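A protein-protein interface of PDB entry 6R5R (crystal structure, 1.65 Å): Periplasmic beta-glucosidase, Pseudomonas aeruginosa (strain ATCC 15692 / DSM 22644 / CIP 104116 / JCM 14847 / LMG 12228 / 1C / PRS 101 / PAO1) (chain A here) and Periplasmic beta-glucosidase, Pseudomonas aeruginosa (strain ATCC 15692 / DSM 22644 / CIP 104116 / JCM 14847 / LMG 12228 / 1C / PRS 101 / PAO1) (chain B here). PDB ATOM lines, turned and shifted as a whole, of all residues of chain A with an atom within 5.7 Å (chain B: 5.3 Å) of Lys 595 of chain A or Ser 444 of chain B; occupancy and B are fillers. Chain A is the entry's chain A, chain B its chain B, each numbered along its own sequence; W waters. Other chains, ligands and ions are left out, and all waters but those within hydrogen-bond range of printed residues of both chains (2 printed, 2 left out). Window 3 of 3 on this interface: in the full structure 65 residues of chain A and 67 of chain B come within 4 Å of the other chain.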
ATOM      1  N   PRO A 593      16.661  -3.436 -32.992  1.00  0.00           N
ATOM      2  CA  PRO A 593      16.779  -4.777 -33.600  1.00  0.00           C
ATOM      3  C   PRO A 593      17.105  -5.830 -32.529  1.00  0.00           C
ATOM      4  O   PRO A 593      17.808  -6.796 -32.782  1.00  0.00           O
ATOM      5  CB  PRO A 593      17.936  -4.599 -34.598  1.00  0.00           C
ATOM      6  CG  PRO A 593      18.261  -3.104 -34.556  1.00  0.00           C
ATOM      7  CD  PRO A 593      17.801  -2.577 -33.210  1.00  0.00           C
ATOM      8  N   GLY A 594      16.543  -5.616 -31.347  1.00  0.00           N
ATOM      9  CA  GLY A 594      16.991  -6.257 -30.101  1.00  0.00           C
ATOM     10  C   GLY A 594      16.445  -7.658 -29.925  1.00  0.00           C
ATOM     11  O   GLY A 594      15.447  -8.075 -30.605  1.00  0.00           O
ATOM     12  N   LYS A 595      17.042  -8.330 -28.945  1.00  0.00           N
ATOM     13  CA  LYS A 595      16.614  -9.670 -28.495  1.00  0.00           C
ATOM     14  C   LYS A 595      15.209  -9.558 -27.902  1.00  0.00           C
ATOM     15  O   LYS A 595      14.405 -10.424 -28.250  1.00  0.00           O
ATOM     16  CB  LYS A 595      17.601 -10.246 -27.478  1.00  0.00           C
ATOM     17  CG  LYS A 595      17.122 -11.482 -26.719  1.00  0.00           C
ATOM     18  CD  LYS A 595      18.197 -12.098 -25.801  1.00  0.00           C
ATOM     19  CE  LYS A 595      18.995 -13.219 -26.456  1.00  0.00           C
ATOM     20  NZ  LYS A 595      20.026 -13.829 -25.576  1.00  0.00           N
ATOM     21  N   TYR A 596      14.932  -8.545 -27.054  1.00  0.00           N
ATOM     22  CA  TYR A 596      13.654  -8.508 -26.281  1.00  0.00           C
ATOM     23  C   TYR A 596      12.580  -7.791 -27.079  1.00  0.00           C
ATOM     24  O   TYR A 596      11.990  -6.780 -26.647  1.00  0.00           O
ATOM     25  CB  TYR A 596      13.862  -8.006 -24.857  1.00  0.00           C
ATOM     26  CG  TYR A 596      14.670  -8.976 -24.044  1.00  0.00           C
ATOM     27  CD1 TYR A 596      14.091 -10.107 -23.496  1.00  0.00           C
ATOM     28  CD2 TYR A 596      16.046  -8.820 -23.899  1.00  0.00           C
ATOM     29  CE1 TYR A 596      14.829 -11.021 -22.749  1.00  0.00           C
ATOM     30  CE2 TYR A 596      16.799  -9.744 -23.190  1.00  0.00           C
ATOM     31  CZ  TYR A 596      16.192 -10.848 -22.615  1.00  0.00           C
ATOM     32  OH  TYR A 596      16.916 -11.743 -21.879  1.00  0.00           O
ATOM     33  N   THR A 597      12.302  -8.345 -28.244  1.00  0.00           N
ATOM     34  CA  THR A 597      11.280  -7.815 -29.153  1.00  0.00           C
ATOM     35  C   THR A 597      10.456  -8.974 -29.675  1.00  0.00           C
ATOM     36  O   THR A 597      10.800 -10.151 -29.465  1.00  0.00           O
ATOM     37  CB  THR A 597      11.908  -7.000 -30.293  1.00  0.00           C
ATOM     38  OG1 THR A 597      12.756  -7.874 -31.069  1.00  0.00           O
ATOM     39  CG2 THR A 597      12.675  -5.783 -29.801  1.00  0.00           C
ATOM     40  N   ARG A 599       9.583 -11.363 -32.187  1.00  0.00           N
ATOM     41  CA  ARG A 599      10.433 -11.906 -33.279  1.00  0.00           C
ATOM     42  C   ARG A 599      10.724 -13.392 -33.072  1.00  0.00           C
ATOM     43  O   ARG A 599      10.470 -13.931 -32.003  1.00  0.00           O
ATOM     44  CB  ARG A 599      11.760 -11.163 -33.346  1.00  0.00           C
ATOM     45  CG  ARG A 599      12.619 -11.423 -32.106  1.00  0.00           C
ATOM     46  CD  ARG A 599      13.922 -10.658 -32.169  1.00  0.00           C
ATOM     47  NE  ARG A 599      14.799 -11.023 -33.304  1.00  0.00           N
ATOM     48  CZ  ARG A 599      15.876 -11.750 -33.217  1.00  0.00           C
ATOM     49  NH1 ARG A 599      16.093 -12.457 -32.135  1.00  0.00           N
ATOM     50  NH2 ARG A 599      16.664 -11.931 -34.260  1.00  0.00           N
ATOM     51  N   LEU B 439      24.176 -18.857 -32.725  1.00  0.00           N
ATOM     52  CA  LEU B 439      25.132 -18.736 -31.607  1.00  0.00           C
ATOM     53  C   LEU B 439      25.268 -17.267 -31.199  1.00  0.00           C
ATOM     54  O   LEU B 439      25.394 -17.034 -29.981  1.00  0.00           O
ATOM     55  CB  LEU B 439      26.472 -19.309 -32.024  1.00  0.00           C
ATOM     56  CG  LEU B 439      26.552 -20.814 -32.263  1.00  0.00           C
ATOM     57  CD1 LEU B 439      27.969 -21.187 -32.693  1.00  0.00           C
ATOM     58  CD2 LEU B 439      26.199 -21.623 -31.042  1.00  0.00           C
ATOM     59  N   ASP B 440      25.310 -16.342 -32.143  1.00  0.00           N
ATOM     60  CA  ASP B 440      25.419 -14.891 -31.843  1.00  0.00           C
ATOM     61  C   ASP B 440      24.238 -14.438 -30.972  1.00  0.00           C
ATOM     62  O   ASP B 440      24.402 -13.699 -29.978  1.00  0.00           O
ATOM     63  CB  ASP B 440      25.472 -14.050 -33.101  1.00  0.00           C
ATOM     64  CG  ASP B 440      26.689 -14.270 -33.973  1.00  0.00           C
ATOM     65  OD1 ASP B 440      27.694 -14.852 -33.464  1.00  0.00           O
ATOM     66  OD2 ASP B 440      26.552 -13.863 -35.159  1.00  0.00           O
ATOM     67  N   TYR B 441      23.045 -14.908 -31.301  1.00  0.00           N
ATOM     68  CA  TYR B 441      21.849 -14.638 -30.487  1.00  0.00           C
ATOM     69  C   TYR B 441      21.993 -15.200 -29.060  1.00  0.00           C
ATOM     70  O   TYR B 441      21.699 -14.509 -28.073  1.00  0.00           O
ATOM     71  CB  TYR B 441      20.634 -15.269 -31.170  1.00  0.00           C
ATOM     72  CG  TYR B 441      19.378 -15.114 -30.381  1.00  0.00           C
ATOM     73  CD1 TYR B 441      18.660 -13.925 -30.485  1.00  0.00           C
ATOM     74  CD2 TYR B 441      18.913 -16.126 -29.562  1.00  0.00           C
ATOM     75  CE1 TYR B 441      17.481 -13.752 -29.780  1.00  0.00           C
ATOM     76  CE2 TYR B 441      17.771 -15.944 -28.816  1.00  0.00           C
ATOM     77  CZ  TYR B 441      17.059 -14.764 -28.950  1.00  0.00           C
ATOM     78  OH  TYR B 441      15.905 -14.596 -28.261  1.00  0.00           O
ATOM     79  N   LEU B 442      22.360 -16.483 -28.928  1.00  0.00           N
ATOM     80  CA  LEU B 442      22.399 -17.169 -27.636  1.00  0.00           C
ATOM     81  C   LEU B 442      23.501 -16.600 -26.735  1.00  0.00           C
ATOM     82  O   LEU B 442      23.317 -16.629 -25.524  1.00  0.00           O
ATOM     83  CB  LEU B 442      22.568 -18.669 -27.841  1.00  0.00           C
ATOM     84  CG  LEU B 442      21.400 -19.332 -28.575  1.00  0.00           C
ATOM     85  CD1 LEU B 442      21.830 -20.732 -28.964  1.00  0.00           C
ATOM     86  CD2 LEU B 442      20.145 -19.324 -27.664  1.00  0.00           C
ATOM     87  N   ASN B 443      24.535 -16.016 -27.325  1.00  0.00           N
ATOM     88  CA  ASN B 443      25.593 -15.351 -26.517  1.00  0.00           C
ATOM     89  C   ASN B 443      25.379 -13.842 -26.412  1.00  0.00           C
ATOM     90  O   ASN B 443      26.267 -13.147 -25.863  1.00  0.00           O
ATOM     91  CB  ASN B 443      26.985 -15.729 -27.028  1.00  0.00           C
ATOM     92  CG  ASN B 443      27.354 -17.127 -26.563  1.00  0.00           C
ATOM     93  OD1 ASN B 443      26.912 -17.557 -25.488  1.00  0.00           O
ATOM     94  ND2 ASN B 443      28.038 -17.887 -27.401  1.00  0.00           N
ATOM     95  N   SER B 444      24.249 -13.309 -26.828  1.00  0.00           N
ATOM     96  CA  SER B 444      23.988 -11.858 -26.725  1.00  0.00           C
ATOM     97  C   SER B 444      23.521 -11.582 -25.274  1.00  0.00           C
ATOM     98  O   SER B 444      22.722 -12.355 -24.691  1.00  0.00           O
ATOM     99  CB  SER B 444      23.027 -11.434 -27.819  1.00  0.00           C
ATOM    100  OG  SER B 444      21.744 -11.779 -27.392  1.00  0.00           O
ATOM    101  N   TYR B 445      24.040 -10.526 -24.676  1.00  0.00           N
ATOM    102  CA  TYR B 445      23.873 -10.085 -23.257  1.00  0.00           C
ATOM    103  C   TYR B 445      24.797 -10.834 -22.312  1.00  0.00           C
ATOM    104  O   TYR B 445      25.491 -10.196 -21.558  1.00  0.00           O
ATOM    105  CB  TYR B 445      22.442 -10.192 -22.727  1.00  0.00           C
ATOM    106  CG  TYR B 445      21.528  -9.156 -23.307  1.00  0.00           C
ATOM    107  CD1 TYR B 445      21.540  -7.857 -22.836  1.00  0.00           C
ATOM    108  CD2 TYR B 445      20.616  -9.489 -24.299  1.00  0.00           C
ATOM    109  CE1 TYR B 445      20.684  -6.900 -23.361  1.00  0.00           C
ATOM    110  CE2 TYR B 445      19.769  -8.535 -24.841  1.00  0.00           C
ATOM    111  CZ  TYR B 445      19.782  -7.248 -24.357  1.00  0.00           C
ATOM    112  OH  TYR B 445      18.921  -6.329 -24.897  1.00  0.00           O
ATOM    113  N   ASN B 446      24.761 -12.160 -22.329  1.00  0.00           N
ATOM    114  CA  ASN B 446      25.555 -13.004 -21.412  1.00  0.00           C
ATOM    115  C   ASN B 446      26.083 -14.179 -22.193  1.00  0.00           C
ATOM    116  O   ASN B 446      25.373 -14.712 -23.026  1.00  0.00           O
ATOM    117  CB  ASN B 446      24.728 -13.543 -20.246  1.00  0.00           C
ATOM    118  CG  ASN B 446      24.360 -12.441 -19.298  1.00  0.00           C
ATOM    119  OD1 ASN B 446      25.220 -11.952 -18.578  1.00  0.00           O
ATOM    120  ND2 ASN B 446      23.124 -11.963 -19.387  1.00  0.00           N
ATOM    121  N   HIS B 485      13.134 -19.500 -23.875  1.00  0.00           N
ATOM    122  CA  HIS B 485      13.120 -18.436 -22.855  1.00  0.00           C
ATOM    123  C   HIS B 485      12.301 -17.250 -23.384  1.00  0.00           C
ATOM    124  O   HIS B 485      11.791 -17.307 -24.520  1.00  0.00           O
ATOM    125  CB  HIS B 485      14.571 -18.195 -22.414  1.00  0.00           C
ATOM    126  CG  HIS B 485      15.123 -16.830 -22.595  1.00  0.00           C
ATOM    127  ND1 HIS B 485      15.781 -16.433 -23.733  1.00  0.00           N
ATOM    128  CD2 HIS B 485      15.138 -15.774 -21.759  1.00  0.00           C
ATOM    129  CE1 HIS B 485      16.186 -15.186 -23.570  1.00  0.00           C
ATOM    130  NE2 HIS B 485      15.783 -14.754 -22.383  1.00  0.00           N
ATOM    131  N   ALA B 487      11.238 -14.185 -25.286  1.00  0.00           N
ATOM    132  CA  ALA B 487      11.570 -13.637 -26.623  1.00  0.00           C
ATOM    133  C   ALA B 487      12.230 -14.683 -27.539  1.00  0.00           C
ATOM    134  O   ALA B 487      12.247 -14.380 -28.760  1.00  0.00           O
ATOM    135  CB  ALA B 487      12.406 -12.415 -26.546  1.00  0.00           C
HETATM  136  O   HOH W   1      16.541  -6.230 -26.505  1.00  0.00           O
HETATM  137  O   HOH W   2      14.405 -12.719 -29.634  1.00  0.00           O
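Tyr 445 of chain B touches Lys 595 of chain A.
Lys 595 of chain A touches Ala 487 of chain B (O to CB, 3.3 Å).
Tyr 596 of chain A touches Tyr 445 of chain B.
NH1 of Arg 599 of chain A touches CE1 of Tyr 441 of chain B, at 3.0 Å.
Arg 599 of chain A touches Ala 487 of chain B (O to O, 3.7 Å).
Of the 10 printed residues of chain B, 5 touch a printed residue of chain A.
Hydrophobic or aromatic side chains of chain B that line the printed part of chain A: Tyr 441, Tyr 445, His 485 and Ala 487.
Hydrophobic or aromatic side chains of chain A within 4 Å of the printed part of chain B: Tyr 596.
Among the printed residues, no Asp or Glu carboxylate lies within 4 Å of a Lys or Arg side-chain nitrogen of the other chain.
Water W2 lies within hydrogen-bond range of the backbone carbonyl oxygen of Lys 595 of chain A (2.7 Å), the side-chain hydroxyl of Tyr 441 of chain B (2.8 Å), the backbone carbonyl oxygen of Ala 487 of chain B (2.9 Å) and the guanidinium group of Arg 599 of chain A (3.0 Å).
Water W1 lies within hydrogen-bond range of N of Tyr 596 of chain A (2.9 Å), OH of Tyr 445 of chain B (2.9 Å) and N of Lys 595 of chain A (3.3 Å).
The backbone carbonyl oxygen (O) of Tyr 441 of chain B is in hydrogen-bond range of the side-chain amino group (NZ) of Lys 595 of chain A (3.1 Å).
The side-chain amino group (NZ) of Lys 595 of chain A lies within hydrogen-bond range of the backbone carbonyl oxygen (O) of Ser 444 of chain B (3.2 Å).
A ring nitrogen (NE2) of His 485 of chain B sits at hydrogen-bond distance from the side-chain hydroxyl (OH) of Tyr 596 of chain A, at 3.3 Å.
O of Tyr 441 of chain B is in hydrogen-bond range of OG of Ser 444 of chain B, at 2.8 Å.
Printed residues of chain B within 4 Å of Lys 595 of chain A: Tyr 441 (3.1 Å), Ser 444 (3.2 Å), Tyr 445 (3.8 Å) and Ala 487 (3.3 Å).
Printed residues of chain B within 4 Å of Tyr 596 of chain A: Tyr 445 (3.6 Å) and His 485 (3.3 Å).
Of the printed residues of chain B, Arg 599 of chain A touches Tyr 441 and Ala 487.
Of the printed residues of chain A, Tyr 441 of chain B touches Lys 595 and Arg 599.
Of the printed residues of chain A, Ser 444 of chain B touches Lys 595 (3.2 Å).
Of the printed residues of chain A, Tyr 445 of chain B touches Lys 595 (3.8 Å) and Tyr 596 (3.6 Å).
Of the printed residues of chain A, His 485 of chain B touches Tyr 596 (3.3 Å).
The nearest printed residue of chain B that does not touch Lys 595 of chain A is His 485 of chain B (4.3 Å).
The nearest printed residue of chain A that does not touch Ser 444 of chain B is Tyr 596 of chain A (6.5 Å).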
